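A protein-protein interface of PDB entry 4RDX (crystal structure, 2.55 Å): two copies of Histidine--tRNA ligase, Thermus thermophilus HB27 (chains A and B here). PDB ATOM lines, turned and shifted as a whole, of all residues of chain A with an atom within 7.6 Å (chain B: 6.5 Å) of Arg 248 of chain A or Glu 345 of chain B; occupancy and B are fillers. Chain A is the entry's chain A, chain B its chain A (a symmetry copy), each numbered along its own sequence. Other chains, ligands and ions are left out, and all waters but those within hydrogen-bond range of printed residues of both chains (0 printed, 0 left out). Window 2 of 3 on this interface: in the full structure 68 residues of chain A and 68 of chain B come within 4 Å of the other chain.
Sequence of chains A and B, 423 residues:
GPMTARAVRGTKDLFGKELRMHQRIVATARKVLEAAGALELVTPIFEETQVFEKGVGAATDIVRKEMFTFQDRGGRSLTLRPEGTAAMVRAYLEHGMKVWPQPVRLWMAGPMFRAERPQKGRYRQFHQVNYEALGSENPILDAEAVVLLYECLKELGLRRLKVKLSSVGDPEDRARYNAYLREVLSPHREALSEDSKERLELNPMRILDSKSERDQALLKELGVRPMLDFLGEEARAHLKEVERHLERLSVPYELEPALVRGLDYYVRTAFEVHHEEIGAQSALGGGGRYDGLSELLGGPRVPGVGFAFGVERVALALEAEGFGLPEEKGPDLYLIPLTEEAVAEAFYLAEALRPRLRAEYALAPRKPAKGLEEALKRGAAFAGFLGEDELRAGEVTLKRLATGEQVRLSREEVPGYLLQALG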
ATOM      1  N   ILE A 140      20.521 -24.840   0.015  1.00  0.00           N
ATOM      2  CA  ILE A 140      21.740 -24.244   0.553  1.00  0.00           C
ATOM      3  C   ILE A 140      22.795 -25.315   0.812  1.00  0.00           C
ATOM      4  O   ILE A 140      23.978 -25.106   0.554  1.00  0.00           O
ATOM      5  CB  ILE A 140      21.453 -23.456   1.854  1.00  0.00           C
ATOM      6  CG1 ILE A 140      20.671 -22.176   1.545  1.00  0.00           C
ATOM      7  CG2 ILE A 140      22.743 -23.125   2.589  1.00  0.00           C
ATOM      8  CD1 ILE A 140      20.457 -21.282   2.748  1.00  0.00           C
ATOM      9  N   VAL A 242      19.565 -23.529  -5.954  1.00  0.00           N
ATOM     10  CA  VAL A 242      20.981 -23.917  -5.953  1.00  0.00           C
ATOM     11  C   VAL A 242      21.823 -23.000  -6.848  1.00  0.00           C
ATOM     12  O   VAL A 242      22.836 -22.435  -6.414  1.00  0.00           O
ATOM     13  CB  VAL A 242      21.178 -25.373  -6.418  1.00  0.00           C
ATOM     14  CG1 VAL A 242      22.660 -25.696  -6.539  1.00  0.00           C
ATOM     15  CG2 VAL A 242      20.497 -26.333  -5.464  1.00  0.00           C
ATOM     16  N   GLU A 243      21.385 -22.855  -8.098  1.00  0.00           N
ATOM     17  CA  GLU A 243      22.053 -22.000  -9.071  1.00  0.00           C
ATOM     18  C   GLU A 243      22.167 -20.571  -8.559  1.00  0.00           C
ATOM     19  O   GLU A 243      23.199 -19.932  -8.730  1.00  0.00           O
ATOM     20  CB  GLU A 243      21.301 -22.003 -10.402  1.00  0.00           C
ATOM     21  CG  GLU A 243      21.269 -23.341 -11.124  1.00  0.00           C
ATOM     22  CD  GLU A 243      20.526 -23.258 -12.443  1.00  0.00           C
ATOM     23  OE1 GLU A 243      20.121 -22.138 -12.820  1.00  0.00           O
ATOM     24  OE2 GLU A 243      20.345 -24.304 -13.102  1.00  0.00           O
ATOM     25  N   ARG A 244      21.100 -20.078  -7.937  1.00  0.00           N
ATOM     26  CA  ARG A 244      21.088 -18.732  -7.375  1.00  0.00           C
ATOM     27  C   ARG A 244      22.194 -18.567  -6.335  1.00  0.00           C
ATOM     28  O   ARG A 244      22.922 -17.562  -6.324  1.00  0.00           O
ATOM     29  CB  ARG A 244      19.728 -18.435  -6.745  1.00  0.00           C
ATOM     30  CG  ARG A 244      19.624 -17.053  -6.133  1.00  0.00           C
ATOM     31  CD  ARG A 244      18.240 -16.797  -5.563  1.00  0.00           C
ATOM     32  NE  ARG A 244      18.316 -16.208  -4.231  1.00  0.00           N
ATOM     33  CZ  ARG A 244      17.895 -16.812  -3.124  1.00  0.00           C
ATOM     34  NH1 ARG A 244      17.350 -18.018  -3.194  1.00  0.00           N
ATOM     35  NH2 ARG A 244      18.007 -16.205  -1.950  1.00  0.00           N
ATOM     36  N   HIS A 245      22.323 -19.564  -5.464  1.00  0.00           N
ATOM     37  CA  HIS A 245      23.371 -19.529  -4.446  1.00  0.00           C
ATOM     38  C   HIS A 245      24.766 -19.558  -5.056  1.00  0.00           C
ATOM     39  O   HIS A 245      25.625 -18.759  -4.681  1.00  0.00           O
ATOM     40  CB  HIS A 245      23.215 -20.676  -3.455  1.00  0.00           C
ATOM     41  CG  HIS A 245      21.997 -20.570  -2.598  1.00  0.00           C
ATOM     42  ND1 HIS A 245      21.621 -19.397  -1.974  1.00  0.00           N
ATOM     43  CD2 HIS A 245      21.069 -21.491  -2.248  1.00  0.00           C
ATOM     44  CE1 HIS A 245      20.516 -19.600  -1.286  1.00  0.00           C
ATOM     45  NE2 HIS A 245      20.158 -20.865  -1.435  1.00  0.00           N
ATOM     46  N   LEU A 246      24.994 -20.480  -5.988  1.00  0.00           N
ATOM     47  CA  LEU A 246      26.288 -20.552  -6.668  1.00  0.00           C
ATOM     48  C   LEU A 246      26.629 -19.247  -7.396  1.00  0.00           C
ATOM     49  O   LEU A 246      27.788 -18.836  -7.436  1.00  0.00           O
ATOM     50  CB  LEU A 246      26.329 -21.733  -7.643  1.00  0.00           C
ATOM     51  CG  LEU A 246      26.239 -23.130  -7.022  1.00  0.00           C
ATOM     52  CD1 LEU A 246      26.330 -24.207  -8.091  1.00  0.00           C
ATOM     53  CD2 LEU A 246      27.319 -23.324  -5.968  1.00  0.00           C
ATOM     54  N   GLU A 247      25.616 -18.594  -7.954  1.00  0.00           N
ATOM     55  CA  GLU A 247      25.814 -17.345  -8.678  1.00  0.00           C
ATOM     56  C   GLU A 247      26.165 -16.206  -7.729  1.00  0.00           C
ATOM     57  O   GLU A 247      26.971 -15.337  -8.062  1.00  0.00           O
ATOM     58  CB  GLU A 247      24.577 -16.995  -9.506  1.00  0.00           C
ATOM     59  CG  GLU A 247      24.414 -17.842 -10.759  1.00  0.00           C
ATOM     60  CD  GLU A 247      23.067 -17.647 -11.421  1.00  0.00           C
ATOM     61  OE1 GLU A 247      22.397 -16.642 -11.111  1.00  0.00           O
ATOM     62  OE2 GLU A 247      22.673 -18.503 -12.242  1.00  0.00           O
ATOM     63  N   ARG A 248      25.558 -16.213  -6.546  1.00  0.00           N
ATOM     64  CA  ARG A 248      25.900 -15.217  -5.534  1.00  0.00           C
ATOM     65  C   ARG A 248      27.354 -15.352  -5.096  1.00  0.00           C
ATOM     66  O   ARG A 248      28.038 -14.356  -4.864  1.00  0.00           O
ATOM     67  CB  ARG A 248      24.980 -15.338  -4.318  1.00  0.00           C
ATOM     68  CG  ARG A 248      25.300 -14.365  -3.180  1.00  0.00           C
ATOM     69  CD  ARG A 248      25.115 -12.905  -3.594  1.00  0.00           C
ATOM     70  NE  ARG A 248      24.709 -12.048  -2.479  1.00  0.00           N
ATOM     71  CZ  ARG A 248      25.542 -11.333  -1.726  1.00  0.00           C
ATOM     72  NH1 ARG A 248      26.848 -11.364  -1.959  1.00  0.00           N
ATOM     73  NH2 ARG A 248      25.069 -10.584  -0.739  1.00  0.00           N
ATOM     74  N   LEU A 249      27.826 -16.590  -4.988  1.00  0.00           N
ATOM     75  CA  LEU A 249      29.176 -16.850  -4.501  1.00  0.00           C
ATOM     76  C   LEU A 249      30.190 -16.842  -5.638  1.00  0.00           C
ATOM     77  O   LEU A 249      31.353 -17.206  -5.446  1.00  0.00           O
ATOM     78  CB  LEU A 249      29.230 -18.181  -3.750  1.00  0.00           C
ATOM     79  CG  LEU A 249      28.486 -18.211  -2.413  1.00  0.00           C
ATOM     80  CD1 LEU A 249      28.440 -19.623  -1.850  1.00  0.00           C
ATOM     81  CD2 LEU A 249      29.130 -17.255  -1.417  1.00  0.00           C
ATOM     82  N   SER A 250      29.732 -16.419  -6.813  1.00  0.00           N
ATOM     83  CA  SER A 250      30.558 -16.354  -8.012  1.00  0.00           C
ATOM     84  C   SER A 250      31.222 -17.681  -8.354  1.00  0.00           C
ATOM     85  O   SER A 250      32.359 -17.704  -8.822  1.00  0.00           O
ATOM     86  CB  SER A 250      31.614 -15.252  -7.893  1.00  0.00           C
ATOM     87  OG  SER A 250      31.030 -13.968  -8.018  1.00  0.00           O
ATOM     88  N   VAL A 251      30.521 -18.784  -8.114  1.00  0.00           N
ATOM     89  CA  VAL A 251      31.042 -20.096  -8.475  1.00  0.00           C
ATOM     90  C   VAL A 251      30.610 -20.450  -9.891  1.00  0.00           C
ATOM     91  O   VAL A 251      29.438 -20.745 -10.130  1.00  0.00           O
ATOM     92  CB  VAL A 251      30.587 -21.197  -7.489  1.00  0.00           C
ATOM     93  CG1 VAL A 251      30.968 -22.580  -8.012  1.00  0.00           C
ATOM     94  CG2 VAL A 251      31.188 -20.956  -6.110  1.00  0.00           C
ATOM     95  N   TYR A 253      30.019 -22.624 -13.151  1.00  0.00           N
ATOM     96  CA  TYR A 253      29.695 -24.024 -13.340  1.00  0.00           C
ATOM     97  C   TYR A 253      29.076 -24.186 -14.713  1.00  0.00           C
ATOM     98  O   TYR A 253      28.311 -23.336 -15.167  1.00  0.00           O
ATOM     99  CB  TYR A 253      28.712 -24.496 -12.265  1.00  0.00           C
ATOM    100  CG  TYR A 253      27.410 -23.722 -12.245  1.00  0.00           C
ATOM    101  CD1 TYR A 253      27.295 -22.542 -11.524  1.00  0.00           C
ATOM    102  CD2 TYR A 253      26.298 -24.171 -12.948  1.00  0.00           C
ATOM    103  CE1 TYR A 253      26.115 -21.828 -11.505  1.00  0.00           C
ATOM    104  CE2 TYR A 253      25.113 -23.463 -12.937  1.00  0.00           C
ATOM    105  CZ  TYR A 253      25.025 -22.293 -12.211  1.00  0.00           C
ATOM    106  OH  TYR A 253      23.847 -21.582 -12.193  1.00  0.00           O
ATOM    107  N   LEU B 335      27.064 -18.396  13.356  1.00  0.00           N
ATOM    108  CA  LEU B 335      26.084 -17.423  12.890  1.00  0.00           C
ATOM    109  C   LEU B 335      24.654 -17.849  13.194  1.00  0.00           C
ATOM    110  O   LEU B 335      24.266 -18.998  12.984  1.00  0.00           O
ATOM    111  CB  LEU B 335      26.257 -17.164  11.391  1.00  0.00           C
ATOM    112  CG  LEU B 335      27.553 -16.466  10.972  1.00  0.00           C
ATOM    113  CD1 LEU B 335      27.761 -16.584   9.470  1.00  0.00           C
ATOM    114  CD2 LEU B 335      27.540 -15.007  11.397  1.00  0.00           C
ATOM    115  N   GLU B 341      15.119 -14.815   5.493  1.00  0.00           N
ATOM    116  CA  GLU B 341      16.035 -14.386   4.441  1.00  0.00           C
ATOM    117  C   GLU B 341      17.467 -14.200   4.931  1.00  0.00           C
ATOM    118  O   GLU B 341      18.385 -14.033   4.129  1.00  0.00           O
ATOM    119  CB  GLU B 341      15.535 -13.093   3.795  1.00  0.00           C
ATOM    120  N   ALA B 342      17.655 -14.223   6.247  1.00  0.00           N
ATOM    121  CA  ALA B 342      18.982 -14.046   6.825  1.00  0.00           C
ATOM    122  C   ALA B 342      19.828 -15.308   6.695  1.00  0.00           C
ATOM    123  O   ALA B 342      21.050 -15.227   6.568  1.00  0.00           O
ATOM    124  CB  ALA B 342      18.875 -13.625   8.283  1.00  0.00           C
ATOM    125  N   VAL B 343      19.165 -16.463   6.735  1.00  0.00           N
ATOM    126  CA  VAL B 343      19.831 -17.761   6.646  1.00  0.00           C
ATOM    127  C   VAL B 343      20.858 -17.794   5.515  1.00  0.00           C
ATOM    128  O   VAL B 343      22.058 -17.963   5.759  1.00  0.00           O
ATOM    129  CB  VAL B 343      18.817 -18.906   6.448  1.00  0.00           C
ATOM    130  CG1 VAL B 343      19.542 -20.222   6.235  1.00  0.00           C
ATOM    131  CG2 VAL B 343      17.883 -19.001   7.643  1.00  0.00           C
ATOM    132  N   ALA B 344      20.377 -17.602   4.289  1.00  0.00           N
ATOM    133  CA  ALA B 344      21.236 -17.547   3.112  1.00  0.00           C
ATOM    134  C   ALA B 344      22.394 -16.582   3.325  1.00  0.00           C
ATOM    135  O   ALA B 344      23.550 -16.915   3.056  1.00  0.00           O
ATOM    136  CB  ALA B 344      20.431 -17.137   1.892  1.00  0.00           C
ATOM    137  N   GLU B 345      22.082 -15.393   3.835  1.00  0.00           N
ATOM    138  CA  GLU B 345      23.111 -14.394   4.086  1.00  0.00           C
ATOM    139  C   GLU B 345      24.191 -14.961   5.000  1.00  0.00           C
ATOM    140  O   GLU B 345      25.381 -14.880   4.675  1.00  0.00           O
ATOM    141  CB  GLU B 345      22.508 -13.115   4.667  1.00  0.00           C
ATOM    142  CG  GLU B 345      21.572 -12.399   3.709  1.00  0.00           C
ATOM    143  CD  GLU B 345      22.243 -12.031   2.395  1.00  0.00           C
ATOM    144  OE1 GLU B 345      23.374 -11.498   2.425  1.00  0.00           O
ATOM    145  OE2 GLU B 345      21.637 -12.280   1.329  1.00  0.00           O
ATOM    146  N   ALA B 346      23.769 -15.571   6.110  1.00  0.00           N
ATOM    147  CA  ALA B 346      24.706 -16.208   7.031  1.00  0.00           C
ATOM    148  C   ALA B 346      25.602 -17.133   6.229  1.00  0.00           C
ATOM    149  O   ALA B 346      26.833 -17.027   6.301  1.00  0.00           O
ATOM    150  CB  ALA B 346      23.968 -16.983   8.117  1.00  0.00           C
ATOM    151  N   PHE B 347      24.969 -17.996   5.429  1.00  0.00           N
ATOM    152  CA  PHE B 347      25.678 -18.945   4.579  1.00  0.00           C
ATOM    153  C   PHE B 347      26.766 -18.200   3.827  1.00  0.00           C
ATOM    154  O   PHE B 347      27.953 -18.493   4.001  1.00  0.00           O
ATOM    155  CB  PHE B 347      24.713 -19.654   3.617  1.00  0.00           C
ATOM    156  CG  PHE B 347      25.394 -20.504   2.578  1.00  0.00           C
ATOM    157  CD1 PHE B 347      26.243 -21.535   2.952  1.00  0.00           C
ATOM    158  CD2 PHE B 347      25.170 -20.283   1.225  1.00  0.00           C
ATOM    159  CE1 PHE B 347      26.871 -22.323   1.995  1.00  0.00           C
ATOM    160  CE2 PHE B 347      25.794 -21.068   0.262  1.00  0.00           C
ATOM    161  CZ  PHE B 347      26.645 -22.088   0.650  1.00  0.00           C
ATOM    162  N   TYR B 348      26.357 -17.180   3.072  1.00  0.00           N
ATOM    163  CA  TYR B 348      27.286 -16.390   2.274  1.00  0.00           C
ATOM    164  C   TYR B 348      28.436 -15.900   3.143  1.00  0.00           C
ATOM    165  O   TYR B 348      29.610 -16.112   2.814  1.00  0.00           O
ATOM    166  CB  TYR B 348      26.569 -15.198   1.629  1.00  0.00           C
ATOM    167  CG  TYR B 348      25.430 -15.584   0.708  1.00  0.00           C
ATOM    168  CD1 TYR B 348      25.403 -16.828   0.090  1.00  0.00           C
ATOM    169  CD2 TYR B 348      24.379 -14.709   0.462  1.00  0.00           C
ATOM    170  CE1 TYR B 348      24.363 -17.189  -0.747  1.00  0.00           C
ATOM    171  CE2 TYR B 348      23.332 -15.063  -0.376  1.00  0.00           C
ATOM    172  CZ  TYR B 348      23.332 -16.303  -0.978  1.00  0.00           C
ATOM    173  OH  TYR B 348      22.299 -16.666  -1.814  1.00  0.00           O
ATOM    174  N   LEU B 349      28.092 -15.281   4.273  1.00  0.00           N
ATOM    175  CA  LEU B 349      29.094 -14.720   5.173  1.00  0.00           C
ATOM    176  C   LEU B 349      30.062 -15.800   5.614  1.00  0.00           C
ATOM    177  O   LEU B 349      31.276 -15.608   5.566  1.00  0.00           O
ATOM    178  CB  LEU B 349      28.445 -14.052   6.389  1.00  0.00           C
ATOM    179  CG  LEU B 349      29.412 -13.410   7.387  1.00  0.00           C
ATOM    180  CD1 LEU B 349      30.389 -12.504   6.673  1.00  0.00           C
ATOM    181  CD2 LEU B 349      28.666 -12.630   8.452  1.00  0.00           C
ATOM    182  N   ALA B 350      29.515 -16.949   6.001  1.00  0.00           N
ATOM    183  CA  ALA B 350      30.343 -18.050   6.466  1.00  0.00           C
ATOM    184  C   ALA B 350      31.329 -18.426   5.369  1.00  0.00           C
ATOM    185  O   ALA B 350      32.519 -18.633   5.633  1.00  0.00           O
ATOM    186  CB  ALA B 350      29.486 -19.239   6.861  1.00  0.00           C
ATOM    187  N   LEU B 386      22.275 -12.137  12.820  1.00  0.00           N
ATOM    188  CA  LEU B 386      21.731 -11.571  11.592  1.00  0.00           C
ATOM    189  C   LEU B 386      20.211 -11.494  11.657  1.00  0.00           C
ATOM    190  O   LEU B 386      19.519 -12.497  11.471  1.00  0.00           O
ATOM    191  CB  LEU B 386      22.153 -12.392  10.372  1.00  0.00           C
ATOM    192  CG  LEU B 386      23.566 -12.202   9.815  1.00  0.00           C
ATOM    193  CD1 LEU B 386      23.780 -13.130   8.636  1.00  0.00           C
ATOM    194  CD2 LEU B 386      23.801 -10.762   9.402  1.00  0.00           C
ATOM    195  N   LEU B 391      20.639  -7.056   8.248  1.00  0.00           N
ATOM    196  CA  LEU B 391      20.375  -7.244   6.825  1.00  0.00           C
ATOM    197  C   LEU B 391      20.101  -5.916   6.133  1.00  0.00           C
ATOM    198  O   LEU B 391      20.480  -5.721   4.977  1.00  0.00           O
ATOM    199  CB  LEU B 391      19.174  -8.169   6.625  1.00  0.00           C
ATOM    200  CG  LEU B 391      19.458  -9.569   6.077  1.00  0.00           C
ATOM    201  CD1 LEU B 391      20.432 -10.316   6.973  1.00  0.00           C
ATOM    202  CD2 LEU B 391      18.163 -10.348   5.918  1.00  0.00           C
ATOM    203  N   ARG B 411      29.522  -5.699   7.062  1.00  0.00           N
ATOM    204  CA  ARG B 411      29.970  -7.018   6.627  1.00  0.00           C
ATOM    205  C   ARG B 411      31.397  -6.994   6.085  1.00  0.00           C
ATOM    206  O   ARG B 411      32.235  -7.813   6.467  1.00  0.00           O
ATOM    207  CB  ARG B 411      29.016  -7.593   5.578  1.00  0.00           C
ATOM    208  CG  ARG B 411      29.397  -8.984   5.108  1.00  0.00           C
ATOM    209  CD  ARG B 411      28.172  -9.763   4.671  1.00  0.00           C
ATOM    210  NE  ARG B 411      26.973  -9.311   5.370  1.00  0.00           N
ATOM    211  CZ  ARG B 411      25.836  -9.997   5.425  1.00  0.00           C
ATOM    212  NH1 ARG B 411      25.744 -11.180   4.833  1.00  0.00           N
ATOM    213  NH2 ARG B 411      24.793  -9.501   6.080  1.00  0.00           N
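Arg 248 of chain A touches just these residues of chain B: Glu 345 (3.7 Å) and Tyr 348 (3.5 Å).
Of chain A, only Arg 248 (3.7 Å) comes within 4 Å of Glu 345 of chain B.
Ala 344 of chain B touches just one residue of chain A: Ile 140 (3.8 Å).
Of the printed residues of chain A, Val 343 of chain B touches Ile 140.
Of the printed residues of chain B, His 245 of chain A touches Tyr 348.
Printed residues of chain B within 4 Å of Ile 140 of chain A: Val 343 (3.8 Å), Ala 344 (3.8 Å) and Phe 347 (3.7 Å).
Printed residues of chain B within 4 Å of Leu 249 of chain A: Phe 347 (3.7 Å).
Of the printed residues of chain A, Phe 347 of chain B touches Ile 140 and Leu 249.
The nearest printed residue of chain A that does not touch Phe 347 of chain B is His 245 of chain A (4.5 Å).
The side-chain carboxylate (OE1) of Glu 345 of chain B is in salt-bridge range of the guanidinium group (NH1) of Arg 411 of chain B.
CD1 of Ile 140 of chain A touches CG1 of Val 343 of chain B, at 3.8 Å.
Ile 140 of chain A touches Ala 344 of chain B (CD1 to CA, 3.8 Å).
Phe 347 of chain B touches Ile 140 of chain A.
Arg 248 of chain A touches Tyr 348 of chain B.
Phe 347 of chain B touches Leu 249 of chain A (CE2 to CD1, 3.7 Å).
Of the 14 printed residues of chain B, 5 touch a printed residue of chain A.
Hydrophobic or aromatic side chains of chain B that line the printed part of chain A: Val 343, Phe 347 and Tyr 348.
Of the 12 printed residues of chain A, 4 touch a printed residue of chain B.
Among the printed residues, Asp or Glu carboxylates within 4 Å of a Lys or Arg side-chain nitrogen of the other chain: Arg 248 of chain A with Glu 345 of chain B (3.7 Å).
No position is printed for both chains.
Of the 7 pairs that touch across the chains among the printed residues, none has its exchanged pair printed and touching as well.
OH of Tyr 348 of chain B lies within hydrogen-bond range of ND1 of His 245 of chain A, at 2.8 Å.
NH2 of Arg 248 of chain A is in salt-bridge range of OE1 of Glu 345 of chain B (3.7 Å).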
